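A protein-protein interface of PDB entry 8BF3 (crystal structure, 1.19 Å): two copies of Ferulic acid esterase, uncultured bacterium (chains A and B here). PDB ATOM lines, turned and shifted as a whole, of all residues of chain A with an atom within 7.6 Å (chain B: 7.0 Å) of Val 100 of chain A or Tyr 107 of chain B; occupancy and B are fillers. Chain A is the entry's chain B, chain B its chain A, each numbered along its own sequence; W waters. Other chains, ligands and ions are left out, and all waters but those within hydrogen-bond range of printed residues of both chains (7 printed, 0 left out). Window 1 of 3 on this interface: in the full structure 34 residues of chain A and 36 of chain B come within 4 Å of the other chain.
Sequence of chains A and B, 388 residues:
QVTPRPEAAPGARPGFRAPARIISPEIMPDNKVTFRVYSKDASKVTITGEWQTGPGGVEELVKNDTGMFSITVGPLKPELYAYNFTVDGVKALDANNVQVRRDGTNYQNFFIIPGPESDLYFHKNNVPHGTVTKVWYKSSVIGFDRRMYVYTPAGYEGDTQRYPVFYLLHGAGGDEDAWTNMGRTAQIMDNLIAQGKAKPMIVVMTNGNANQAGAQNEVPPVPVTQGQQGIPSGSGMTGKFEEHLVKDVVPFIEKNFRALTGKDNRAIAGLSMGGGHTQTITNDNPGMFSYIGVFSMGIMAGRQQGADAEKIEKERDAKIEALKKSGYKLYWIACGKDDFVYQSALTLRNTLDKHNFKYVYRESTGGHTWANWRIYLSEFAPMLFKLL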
ATOM      1  N   LEU A  93      -2.334   3.507  33.058  1.00  0.00           N
ATOM      2  CA  LEU A  93      -2.141   3.880  31.677  1.00  0.00           C
ATOM      3  C   LEU A  93      -1.162   2.928  30.997  1.00  0.00           C
ATOM      4  O   LEU A  93      -0.533   2.072  31.621  1.00  0.00           O
ATOM      5  CB  LEU A  93      -1.635   5.315  31.590  1.00  0.00           C
ATOM      6  CG  LEU A  93      -2.579   6.375  32.159  1.00  0.00           C
ATOM      7  CD1 LEU A  93      -1.955   7.768  32.076  1.00  0.00           C
ATOM      8  CD2 LEU A  93      -3.927   6.342  31.460  1.00  0.00           C
ATOM      9  N   ASP A  94      -1.053   3.091  29.689  1.00  0.00           N
ATOM     10  CA  ASP A  94      -0.189   2.284  28.835  1.00  0.00           C
ATOM     11  C   ASP A  94       1.161   2.976  28.794  1.00  0.00           C
ATOM     12  O   ASP A  94       1.318   4.010  28.143  1.00  0.00           O
ATOM     13  CB  ASP A  94      -0.818   2.209  27.449  1.00  0.00           C
ATOM     14  CG  ASP A  94      -0.137   1.238  26.533  1.00  0.00           C
ATOM     15  OD1 ASP A  94       1.048   0.924  26.780  1.00  0.00           O
ATOM     16  OD2 ASP A  94      -0.808   0.819  25.557  1.00  0.00           O
ATOM     17  N   ALA A  95       2.130   2.428  29.526  1.00  0.00           N
ATOM     18  CA  ALA A  95       3.440   3.050  29.609  1.00  0.00           C
ATOM     19  C   ALA A  95       4.191   3.019  28.288  1.00  0.00           C
ATOM     20  O   ALA A  95       5.203   3.704  28.155  1.00  0.00           O
ATOM     21  CB  ALA A  95       4.252   2.374  30.713  1.00  0.00           C
ATOM     22  N   ASN A  97       2.697   3.853  25.369  1.00  0.00           N
ATOM     23  CA  ASN A  97       2.002   4.774  24.478  1.00  0.00           C
ATOM     24  C   ASN A  97       2.189   6.201  24.977  1.00  0.00           C
ATOM     25  O   ASN A  97       1.615   6.585  25.999  1.00  0.00           O
ATOM     26  CB  ASN A  97       0.518   4.419  24.431  1.00  0.00           C
ATOM     27  CG  ASN A  97      -0.239   5.273  23.464  1.00  0.00           C
ATOM     28  OD1 ASN A  97       0.333   6.148  22.806  1.00  0.00           O
ATOM     29  ND2 ASN A  97      -1.529   5.036  23.358  1.00  0.00           N
ATOM     30  N   VAL A  98       2.966   6.995  24.241  1.00  0.00           N
ATOM     31  CA  VAL A  98       3.229   8.369  24.643  1.00  0.00           C
ATOM     32  C   VAL A  98       2.021   9.285  24.500  1.00  0.00           C
ATOM     33  O   VAL A  98       2.024  10.397  25.043  1.00  0.00           O
ATOM     34  CB  VAL A  98       4.437   8.900  23.847  1.00  0.00           C
ATOM     35  CG1 VAL A  98       4.055   9.209  22.403  1.00  0.00           C
ATOM     36  CG2 VAL A  98       5.040  10.101  24.531  1.00  0.00           C
ATOM     37  N   GLN A  99       0.981   8.854  23.795  1.00  0.00           N
ATOM     38  CA  GLN A  99      -0.191   9.696  23.576  1.00  0.00           C
ATOM     39  C   GLN A  99      -1.120   9.593  24.778  1.00  0.00           C
ATOM     40  O   GLN A  99      -1.705   8.533  25.041  1.00  0.00           O
ATOM     41  CB  GLN A  99      -0.897   9.286  22.293  1.00  0.00           C
ATOM     42  CG  GLN A  99      -0.006   9.433  21.074  1.00  0.00           C
ATOM     43  CD  GLN A  99      -0.757   9.245  19.781  1.00  0.00           C
ATOM     44  OE1 GLN A  99      -1.071   8.118  19.381  1.00  0.00           O
ATOM     45  NE2 GLN A  99      -1.069  10.343  19.128  1.00  0.00           N
ATOM     46  N   VAL A 100      -1.265  10.706  25.492  1.00  0.00           N
ATOM     47  CA  VAL A 100      -2.062  10.809  26.709  1.00  0.00           C
ATOM     48  C   VAL A 100      -2.866  12.088  26.596  1.00  0.00           C
ATOM     49  O   VAL A 100      -2.315  13.137  26.241  1.00  0.00           O
ATOM     50  CB  VAL A 100      -1.155  10.879  27.952  1.00  0.00           C
ATOM     51  CG1 VAL A 100      -1.970  11.095  29.217  1.00  0.00           C
ATOM     52  CG2 VAL A 100      -0.338   9.620  28.090  1.00  0.00           C
ATOM     53  N   ARG A 101      -4.156  12.015  26.895  1.00  0.00           N
ATOM     54  CA  ARG A 101      -5.027  13.183  26.947  1.00  0.00           C
ATOM     55  C   ARG A 101      -5.538  13.360  28.373  1.00  0.00           C
ATOM     56  O   ARG A 101      -5.461  12.455  29.202  1.00  0.00           O
ATOM     57  CB  ARG A 101      -6.215  13.058  25.984  1.00  0.00           C
ATOM     58  CG  ARG A 101      -7.260  12.065  26.422  1.00  0.00           C
ATOM     59  CD  ARG A 101      -8.381  11.950  25.418  1.00  0.00           C
ATOM     60  NE  ARG A 101      -9.536  11.302  26.022  1.00  0.00           N
ATOM     61  CZ  ARG A 101     -10.648  11.002  25.370  1.00  0.00           C
ATOM     62  NH1 ARG A 101     -10.787  11.276  24.086  1.00  0.00           N
ATOM     63  NH2 ARG A 101     -11.632  10.385  26.016  1.00  0.00           N
ATOM     64  N   ARG A 102      -6.097  14.543  28.639  1.00  0.00           N
ATOM     65  CA  ARG A 102      -6.648  14.882  29.945  1.00  0.00           C
ATOM     66  C   ARG A 102      -8.021  15.503  29.781  1.00  0.00           C
ATOM     67  O   ARG A 102      -8.168  16.494  29.064  1.00  0.00           O
ATOM     68  CB  ARG A 102      -5.759  15.886  30.686  1.00  0.00           C
ATOM     69  CG  ARG A 102      -6.262  16.247  32.071  1.00  0.00           C
ATOM     70  CD  ARG A 102      -5.459  17.350  32.726  1.00  0.00           C
ATOM     71  NE  ARG A 102      -5.514  18.587  31.960  1.00  0.00           N
ATOM     72  CZ  ARG A 102      -6.463  19.510  32.053  1.00  0.00           C
ATOM     73  NH1 ARG A 102      -7.431  19.430  32.946  1.00  0.00           N
ATOM     74  NH2 ARG A 102      -6.413  20.569  31.254  1.00  0.00           N
ATOM     75  N   ASN A 106      -9.315  13.352  34.530  1.00  0.00           N
ATOM     76  CA  ASN A 106      -9.269  11.994  33.990  1.00  0.00           C
ATOM     77  C   ASN A 106      -8.248  11.914  32.858  1.00  0.00           C
ATOM     78  O   ASN A 106      -8.466  12.461  31.773  1.00  0.00           O
ATOM     79  CB  ASN A 106     -10.658  11.581  33.508  1.00  0.00           C
ATOM     80  CG  ASN A 106     -10.692  10.169  32.907  1.00  0.00           C
ATOM     81  OD1 ASN A 106      -9.790   9.382  33.101  1.00  0.00           O
ATOM     82  ND2 ASN A 106     -11.730   9.870  32.161  1.00  0.00           N
ATOM     83  N   TYR A 107      -7.140  11.228  33.109  1.00  0.00           N
ATOM     84  CA  TYR A 107      -6.141  10.980  32.084  1.00  0.00           C
ATOM     85  C   TYR A 107      -6.374   9.625  31.431  1.00  0.00           C
ATOM     86  O   TYR A 107      -6.659   8.636  32.113  1.00  0.00           O
ATOM     87  CB  TYR A 107      -4.741  10.981  32.695  1.00  0.00           C
ATOM     88  CG  TYR A 107      -4.267  12.322  33.221  1.00  0.00           C
ATOM     89  CD1 TYR A 107      -4.549  12.728  34.510  1.00  0.00           C
ATOM     90  CD2 TYR A 107      -3.526  13.178  32.427  1.00  0.00           C
ATOM     91  CE1 TYR A 107      -4.109  13.946  34.985  1.00  0.00           C
ATOM     92  CE2 TYR A 107      -3.077  14.387  32.901  1.00  0.00           C
ATOM     93  CZ  TYR A 107      -3.368  14.766  34.171  1.00  0.00           C
ATOM     94  OH  TYR A 107      -2.907  15.982  34.628  1.00  0.00           O
ATOM     95  N   GLN A 108      -6.253   9.582  30.107  1.00  0.00           N
ATOM     96  CA  GLN A 108      -6.337   8.337  29.357  1.00  0.00           C
ATOM     97  C   GLN A 108      -5.343   8.377  28.211  1.00  0.00           C
ATOM     98  O   GLN A 108      -4.989   9.445  27.715  1.00  0.00           O
ATOM     99  CB  GLN A 108      -7.729   8.094  28.773  1.00  0.00           C
ATOM    100  CG  GLN A 108      -8.767   7.706  29.808  1.00  0.00           C
ATOM    101  CD  GLN A 108     -10.051   7.282  29.173  1.00  0.00           C
ATOM    102  OE1 GLN A 108     -10.764   8.105  28.637  1.00  0.00           O
ATOM    103  NE2 GLN A 108     -10.335   5.982  29.195  1.00  0.00           N
ATOM    104  N   ASN A 109      -4.911   7.202  27.775  1.00  0.00           N
ATOM    105  CA  ASN A 109      -4.181   7.129  26.523  1.00  0.00           C
ATOM    106  C   ASN A 109      -5.145   7.272  25.356  1.00  0.00           C
ATOM    107  O   ASN A 109      -6.361   7.135  25.504  1.00  0.00           O
ATOM    108  CB  ASN A 109      -3.476   5.787  26.409  1.00  0.00           C
ATOM    109  CG  ASN A 109      -2.392   5.628  27.422  1.00  0.00           C
ATOM    110  OD1 ASN A 109      -2.585   4.976  28.439  1.00  0.00           O
ATOM    111  ND2 ASN A 109      -1.242   6.218  27.157  1.00  0.00           N
ATOM    112  N   PHE A 110      -4.587   7.482  24.166  1.00  0.00           N
ATOM    113  CA  PHE A 110      -5.403   7.427  22.967  1.00  0.00           C
ATOM    114  C   PHE A 110      -4.571   6.968  21.780  1.00  0.00           C
ATOM    115  O   PHE A 110      -3.340   6.911  21.827  1.00  0.00           O
ATOM    116  CB  PHE A 110      -6.100   8.775  22.675  1.00  0.00           C
ATOM    117  CG  PHE A 110      -5.167   9.904  22.312  1.00  0.00           C
ATOM    118  CD1 PHE A 110      -4.593  10.692  23.302  1.00  0.00           C
ATOM    119  CD2 PHE A 110      -4.878  10.191  20.986  1.00  0.00           C
ATOM    120  CE1 PHE A 110      -3.745  11.746  22.976  1.00  0.00           C
ATOM    121  CE2 PHE A 110      -4.037  11.253  20.655  1.00  0.00           C
ATOM    122  CZ  PHE A 110      -3.469  12.023  21.653  1.00  0.00           C
ATOM    123  N   PHE A 111      -5.274   6.649  20.701  1.00  0.00           N
ATOM    124  CA  PHE A 111      -4.670   6.363  19.413  1.00  0.00           C
ATOM    125  C   PHE A 111      -5.686   6.760  18.360  1.00  0.00           C
ATOM    126  O   PHE A 111      -6.869   6.943  18.651  1.00  0.00           O
ATOM    127  CB  PHE A 111      -4.271   4.885  19.266  1.00  0.00           C
ATOM    128  CG  PHE A 111      -5.427   3.930  19.429  1.00  0.00           C
ATOM    129  CD1 PHE A 111      -6.186   3.539  18.343  1.00  0.00           C
ATOM    130  CD2 PHE A 111      -5.774   3.458  20.677  1.00  0.00           C
ATOM    131  CE1 PHE A 111      -7.258   2.691  18.502  1.00  0.00           C
ATOM    132  CE2 PHE A 111      -6.847   2.612  20.840  1.00  0.00           C
ATOM    133  CZ  PHE A 111      -7.586   2.223  19.754  1.00  0.00           C
ATOM    134  N   ASN A 181      -6.764  19.712  23.673  1.00  0.00           N
ATOM    135  CA  ASN A 181      -6.341  18.407  24.180  1.00  0.00           C
ATOM    136  C   ASN A 181      -7.352  17.325  23.803  1.00  0.00           C
ATOM    137  O   ASN A 181      -7.031  16.384  23.071  1.00  0.00           O
ATOM    138  CB  ASN A 181      -6.190  18.539  25.697  1.00  0.00           C
ATOM    139  CG  ASN A 181      -5.469  17.397  26.330  1.00  0.00           C
ATOM    140  OD1 ASN A 181      -5.636  16.251  25.949  1.00  0.00           O
ATOM    141  ND2 ASN A 181      -4.718  17.698  27.373  1.00  0.00           N
ATOM    142  N   ARG A 184      -8.740  18.109  19.733  1.00  0.00           N
ATOM    143  CA  ARG A 184      -7.834  18.129  18.585  1.00  0.00           C
ATOM    144  C   ARG A 184      -7.981  19.400  17.753  1.00  0.00           C
ATOM    145  O   ARG A 184      -7.756  19.392  16.539  1.00  0.00           O
ATOM    146  CB  ARG A 184      -7.978  16.879  17.705  1.00  0.00           C
ATOM    147  CG  ARG A 184      -7.836  15.551  18.441  1.00  0.00           C
ATOM    148  CD  ARG A 184      -6.429  15.329  18.994  1.00  0.00           C
ATOM    149  NE  ARG A 184      -5.457  15.034  17.947  1.00  0.00           N
ATOM    150  CZ  ARG A 184      -4.166  14.847  18.177  1.00  0.00           C
ATOM    151  NH1 ARG A 184      -3.665  14.982  19.391  1.00  0.00           N
ATOM    152  NH2 ARG A 184      -3.365  14.507  17.170  1.00  0.00           N
ATOM    153  N   TYR B  83       6.896  10.971  41.431  1.00  0.00           N
ATOM    154  CA  TYR B  83       6.700   9.605  41.899  1.00  0.00           C
ATOM    155  C   TYR B  83       5.726   8.874  40.988  1.00  0.00           C
ATOM    156  O   TYR B  83       5.014   9.474  40.178  1.00  0.00           O
ATOM    157  CB  TYR B  83       6.179   9.571  43.351  1.00  0.00           C
ATOM    158  CG  TYR B  83       4.744  10.029  43.495  1.00  0.00           C
ATOM    159  CD1 TYR B  83       4.424  11.375  43.505  1.00  0.00           C
ATOM    160  CD2 TYR B  83       3.706   9.109  43.620  1.00  0.00           C
ATOM    161  CE1 TYR B  83       3.112  11.794  43.611  1.00  0.00           C
ATOM    162  CE2 TYR B  83       2.387   9.515  43.750  1.00  0.00           C
ATOM    163  CZ  TYR B  83       2.094  10.868  43.742  1.00  0.00           C
ATOM    164  OH  TYR B  83       0.800  11.337  43.856  1.00  0.00           O
ATOM    165  N   ASN B  84       5.674   7.557  41.178  1.00  0.00           N
ATOM    166  CA  ASN B  84       4.622   6.712  40.631  1.00  0.00           C
ATOM    167  C   ASN B  84       4.509   5.488  41.527  1.00  0.00           C
ATOM    168  O   ASN B  84       5.357   5.245  42.384  1.00  0.00           O
ATOM    169  CB  ASN B  84       4.887   6.302  39.174  1.00  0.00           C
ATOM    170  CG  ASN B  84       6.187   5.577  38.992  1.00  0.00           C
ATOM    171  OD1 ASN B  84       7.206   6.196  38.709  1.00  0.00           O
ATOM    172  ND2 ASN B  84       6.175   4.259  39.165  1.00  0.00           N
ATOM    173  N   LYS B  91       3.643  -0.388  36.297  1.00  0.00           N
ATOM    174  CA  LYS B  91       3.626   1.029  36.642  1.00  0.00           C
ATOM    175  C   LYS B  91       2.204   1.575  36.640  1.00  0.00           C
ATOM    176  O   LYS B  91       1.415   1.304  35.732  1.00  0.00           O
ATOM    177  CB  LYS B  91       4.444   1.803  35.611  1.00  0.00           C
ATOM    178  CG  LYS B  91       4.492   3.299  35.865  1.00  0.00           C
ATOM    179  CD  LYS B  91       5.461   3.995  34.931  1.00  0.00           C
ATOM    180  CE  LYS B  91       5.521   5.494  35.202  1.00  0.00           C
ATOM    181  NZ  LYS B  91       6.547   6.179  34.374  1.00  0.00           N
ATOM    182  N   LEU B  93       0.165   5.415  37.696  1.00  0.00           N
ATOM    183  CA  LEU B  93       0.144   6.745  38.266  1.00  0.00           C
ATOM    184  C   LEU B  93      -0.921   6.837  39.357  1.00  0.00           C
ATOM    185  O   LEU B  93      -1.720   5.923  39.579  1.00  0.00           O
ATOM    186  CB  LEU B  93      -0.091   7.794  37.179  1.00  0.00           C
ATOM    187  CG  LEU B  93       0.977   7.864  36.093  1.00  0.00           C
ATOM    188  CD1 LEU B  93       0.646   8.949  35.087  1.00  0.00           C
ATOM    189  CD2 LEU B  93       2.343   8.108  36.684  1.00  0.00           C
ATOM    190  N   VAL B 100       0.827  15.894  36.850  1.00  0.00           N
ATOM    191  CA  VAL B 100       1.526  14.897  36.051  1.00  0.00           C
ATOM    192  C   VAL B 100       2.528  15.641  35.185  1.00  0.00           C
ATOM    193  O   VAL B 100       2.180  16.654  34.566  1.00  0.00           O
ATOM    194  CB  VAL B 100       0.551  14.100  35.162  1.00  0.00           C
ATOM    195  CG1 VAL B 100       1.314  13.131  34.282  1.00  0.00           C
ATOM    196  CG2 VAL B 100      -0.474  13.365  35.997  1.00  0.00           C
ATOM    197  N   ARG B 101       3.761  15.151  35.144  1.00  0.00           N
ATOM    198  CA  ARG B 101       4.815  15.689  34.289  1.00  0.00           C
ATOM    199  C   ARG B 101       5.239  14.622  33.287  1.00  0.00           C
ATOM    200  O   ARG B 101       4.928  13.434  33.441  1.00  0.00           O
ATOM    201  CB  ARG B 101       6.024  16.161  35.104  1.00  0.00           C
ATOM    202  CG  ARG B 101       6.856  15.019  35.653  1.00  0.00           C
ATOM    203  CD  ARG B 101       8.014  15.517  36.478  1.00  0.00           C
ATOM    204  NE  ARG B 101       8.989  14.456  36.678  1.00  0.00           N
ATOM    205  CZ  ARG B 101      10.084  14.573  37.407  1.00  0.00           C
ATOM    206  NH1 ARG B 101      10.393  15.709  38.003  1.00  0.00           N
ATOM    207  NH2 ARG B 101      10.878  13.517  37.552  1.00  0.00           N
ATOM    208  N   ARG B 102       5.982  15.056  32.271  1.00  0.00           N
ATOM    209  CA  ARG B 102       6.478  14.168  31.229  1.00  0.00           C
ATOM    210  C   ARG B 102       7.942  14.466  30.954  1.00  0.00           C
ATOM    211  O   ARG B 102       8.291  15.610  30.654  1.00  0.00           O
ATOM    212  CB  ARG B 102       5.688  14.344  29.926  1.00  0.00           C
ATOM    213  CG  ARG B 102       6.129  13.443  28.798  1.00  0.00           C
ATOM    214  CD  ARG B 102       5.459  13.742  27.480  1.00  0.00           C
ATOM    215  NE  ARG B 102       5.751  15.085  26.997  1.00  0.00           N
ATOM    216  CZ  ARG B 102       6.813  15.424  26.276  1.00  0.00           C
ATOM    217  NH1 ARG B 102       7.682  14.523  25.846  1.00  0.00           N
ATOM    218  NH2 ARG B 102       7.008  16.702  25.973  1.00  0.00           N
ATOM    219  N   ASP B 103       8.788  13.440  31.017  1.00  0.00           N
ATOM    220  CA  ASP B 103      10.204  13.508  30.646  1.00  0.00           C
ATOM    221  C   ASP B 103      10.358  12.567  29.454  1.00  0.00           C
ATOM    222  O   ASP B 103      10.514  11.357  29.633  1.00  0.00           O
ATOM    223  CB  ASP B 103      11.064  13.044  31.825  1.00  0.00           C
ATOM    224  CG  ASP B 103      12.560  13.129  31.552  1.00  0.00           C
ATOM    225  OD1 ASP B 103      12.978  13.561  30.458  1.00  0.00           O
ATOM    226  OD2 ASP B 103      13.340  12.778  32.469  1.00  0.00           O
ATOM    227  N   GLY B 104      10.259  13.105  28.236  1.00  0.00           N
ATOM    228  CA  GLY B 104      10.308  12.259  27.063  1.00  0.00           C
ATOM    229  C   GLY B 104       9.100  11.356  26.971  1.00  0.00           C
ATOM    230  O   GLY B 104       7.986  11.820  26.700  1.00  0.00           O
ATOM    231  N   THR B 105       9.302  10.063  27.202  1.00  0.00           N
ATOM    232  CA  THR B 105       8.193   9.122  27.274  1.00  0.00           C
ATOM    233  C   THR B 105       7.802   8.748  28.702  1.00  0.00           C
ATOM    234  O   THR B 105       6.868   7.961  28.883  1.00  0.00           O
ATOM    235  CB  THR B 105       8.527   7.834  26.518  1.00  0.00           C
ATOM    236  OG1 THR B 105       9.728   7.281  27.062  1.00  0.00           O
ATOM    237  CG2 THR B 105       8.705   8.094  25.029  1.00  0.00           C
ATOM    238  N   ASN B 106       8.482   9.280  29.713  1.00  0.00           N
ATOM    239  CA  ASN B 106       8.281   8.878  31.106  1.00  0.00           C
ATOM    240  C   ASN B 106       7.341   9.864  31.792  1.00  0.00           C
ATOM    241  O   ASN B 106       7.720  11.004  32.077  1.00  0.00           O
ATOM    242  CB  ASN B 106       9.630   8.819  31.826  1.00  0.00           C
ATOM    243  CG  ASN B 106       9.513   8.434  33.307  1.00  0.00           C
ATOM    244  OD1 ASN B 106       8.422   8.308  33.858  1.00  0.00           O
ATOM    245  ND2 ASN B 106      10.658   8.275  33.956  1.00  0.00           N
ATOM    246  N   TYR B 107       6.120   9.423  32.071  1.00  0.00           N
ATOM    247  CA  TYR B 107       5.158  10.221  32.816  1.00  0.00           C
ATOM    248  C   TYR B 107       5.222   9.852  34.295  1.00  0.00           C
ATOM    249  O   TYR B 107       5.274   8.674  34.658  1.00  0.00           O
ATOM    250  CB  TYR B 107       3.743   9.966  32.313  1.00  0.00           C
ATOM    251  CG  TYR B 107       3.457  10.469  30.923  1.00  0.00           C
ATOM    252  CD1 TYR B 107       3.723   9.691  29.809  1.00  0.00           C
ATOM    253  CD2 TYR B 107       2.898  11.715  30.731  1.00  0.00           C
ATOM    254  CE1 TYR B 107       3.435  10.138  28.534  1.00  0.00           C
ATOM    255  CE2 TYR B 107       2.609  12.181  29.464  1.00  0.00           C
ATOM    256  CZ  TYR B 107       2.875  11.392  28.365  1.00  0.00           C
ATOM    257  OH  TYR B 107       2.544  11.895  27.125  1.00  0.00           O
ATOM    258  N   GLN B 108       5.181  10.862  35.162  1.00  0.00           N
ATOM    259  CA  GLN B 108       5.124  10.644  36.601  1.00  0.00           C
ATOM    260  C   GLN B 108       4.256  11.712  37.229  1.00  0.00           C
ATOM    261  O   GLN B 108       4.115  12.806  36.683  1.00  0.00           O
ATOM    262  CB  GLN B 108       6.500  10.722  37.242  1.00  0.00           C
ATOM    263  CG  GLN B 108       7.373   9.528  36.939  1.00  0.00           C
ATOM    264  CD  GLN B 108       8.654   9.603  37.689  1.00  0.00           C
ATOM    265  OE1 GLN B 108       9.484  10.441  37.384  1.00  0.00           O
ATOM    266  NE2 GLN B 108       8.826   8.740  38.698  1.00  0.00           N
ATOM    267  N   ASN B 109       3.673  11.393  38.377  1.00  0.00           N
ATOM    268  CA  ASN B 109       3.041  12.428  39.171  1.00  0.00           C
ATOM    269  C   ASN B 109       4.097  13.256  39.886  1.00  0.00           C
ATOM    270  O   ASN B 109       5.260  12.866  39.987  1.00  0.00           O
ATOM    271  CB  ASN B 109       2.148  11.800  40.232  1.00  0.00           C
ATOM    272  CG  ASN B 109       0.981  11.067  39.649  1.00  0.00           C
ATOM    273  OD1 ASN B 109       1.003   9.848  39.532  1.00  0.00           O
ATOM    274  ND2 ASN B 109      -0.055  11.800  39.291  1.00  0.00           N
ATOM    275  N   ASN B 181       7.836  21.911  31.438  1.00  0.00           N
ATOM    276  CA  ASN B 181       7.170  20.784  32.087  1.00  0.00           C
ATOM    277  C   ASN B 181       8.016  20.250  33.241  1.00  0.00           C
ATOM    278  O   ASN B 181       7.622  20.325  34.411  1.00  0.00           O
ATOM    279  CB  ASN B 181       6.909  19.728  31.007  1.00  0.00           C
ATOM    280  CG  ASN B 181       5.965  18.643  31.449  1.00  0.00           C
ATOM    281  OD1 ASN B 181       5.964  18.221  32.601  1.00  0.00           O
ATOM    282  ND2 ASN B 181       5.195  18.141  30.514  1.00  0.00           N
ATOM    283  N   ASN B 217       5.377  13.554  22.041  1.00  0.00           N
ATOM    284  CA  ASN B 217       4.030  13.270  22.518  1.00  0.00           C
ATOM    285  C   ASN B 217       2.958  13.919  21.665  1.00  0.00           C
ATOM    286  O   ASN B 217       1.785  13.553  21.790  1.00  0.00           O
ATOM    287  CB  ASN B 217       3.854  13.696  23.974  1.00  0.00           C
ATOM    288  CG  ASN B 217       3.957  15.189  24.161  1.00  0.00           C
ATOM    289  OD1 ASN B 217       4.823  15.837  23.588  1.00  0.00           O
ATOM    290  ND2 ASN B 217       3.084  15.739  24.978  1.00  0.00           N
HETATM  291  O   HOH W   1       4.969   6.993  27.220  1.00  0.00           O
HETATM  292  O   HOH W   2       0.104  12.605  19.532  1.00  0.00           O
HETATM  293  O   HOH W   3      -0.019  13.098  23.999  1.00  0.00           O
HETATM  294  O   HOH W   4       6.880   4.849  30.000  1.00  0.00           O
HETATM  295  O   HOH W   5      -1.040   5.093  35.081  1.00  0.00           O
HETATM  296  O   HOH W   6       1.584   2.423  33.292  1.00  0.00           O
HETATM  297  O   HOH W   7      -1.128  15.065  20.719  1.00  0.00           O
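OD1 of Asn 217 of chain B is in hydrogen-bond range of NH2 of Arg 102 of chain B, at 3.3 Å.
NZ of Lys 91 of chain B sits at hydrogen-bond distance from O of Tyr 107 of chain B, at 2.8 Å.
Val 100 of chain A touches Tyr 107 of chain B, and with the chains exchanged Tyr 107 of chain A touches Val 100 of chain B.
Positions printed for both chains: 93, 100, 101, 102, 106, 107, 108, 109 and 181.
Of the printed residues of chain B, Val 98 of chain A touches Tyr 107 (2.6 Å) and Asn 217 (3.8 Å).
Of the printed residues of chain B, Val 100 of chain A touches Tyr 107.
Of the printed residues of chain B, Tyr 107 of chain A touches Val 100 (3.7 Å).
Tyr 83 of chain B touches none of the printed residues of chain A.
Printed residues of chain A within 4 Å of Val 100 of chain B: Tyr 107.
Tyr 107 of chain B touches just these residues of chain A: Val 98 and Val 100.
Of the printed residues of chain A, Asn 217 of chain B touches Val 98 (3.8 Å).
The nearest residue of chain A that does not touch Tyr 107 of chain B is Asn 97 of chain A (4.7 Å).
The nearest printed residue of chain B that does not touch Val 98 of chain A is Gly 104 of chain B (4.04 Å).
OH of Tyr 107 of chain B sits at hydrogen-bond distance from O of Val 98 of chain A.
Among the printed residues, merely in contact across the chains: Val 98 of chain A with Asn 217 of chain B (3.8 Å), Val 100 of chain A with Tyr 107 of chain B (3.7 Å) and Tyr 107 of chain A with Val 100 of chain B (3.7 Å).
Of the 16 printed residues of chain B, 3 touch a printed residue of chain A.
Printed residues of chain B that touch a printed residue of chain A: Val 100, Tyr 107 and Asn 217.
Hydrophobic or aromatic side chains of chain B within 4 Å of the printed part of chain A: Val 100 and Tyr 107.
Printed residues of chain A that touch a printed residue of chain B: Val 98, Val 100 and Tyr 107.
Among the printed residues, 4 pairs touch across the chains.
Water W6 bridges the backbone carbonyl oxygen of Lys 91 of chain B (2.7 Å) and the backbone carbonyl oxygen of Leu 93 of chain A (2.7 Å).
Water W1 bridges the backbone carbonyl oxygen of Thr 105 of chain B (2.7 Å) and the backbone carbonyl oxygen of Ala 95 of chain A (3.4 Å).
Water W4 lies within hydrogen-bond range of O of Ala 95 of chain A (2.7 Å) and O of Thr 105 of chain B (3.3 Å).
Water W7 bridges the guanidinium group (NH1) of Arg 184 of chain A (2.9 Å) and the backbone carbonyl oxygen (O) of Asn 217 of chain B (3.5 Å).
Water W5 lies within hydrogen-bond range of N of Leu 93 of chain A (2.9 Å) and N of Leu 93 of chain B (2.9 Å).
Water W3 bridges the backbone carbonyl oxygen (O) of Asn 217 of chain B and the backbone NH (N) of Val 100 of chain A.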
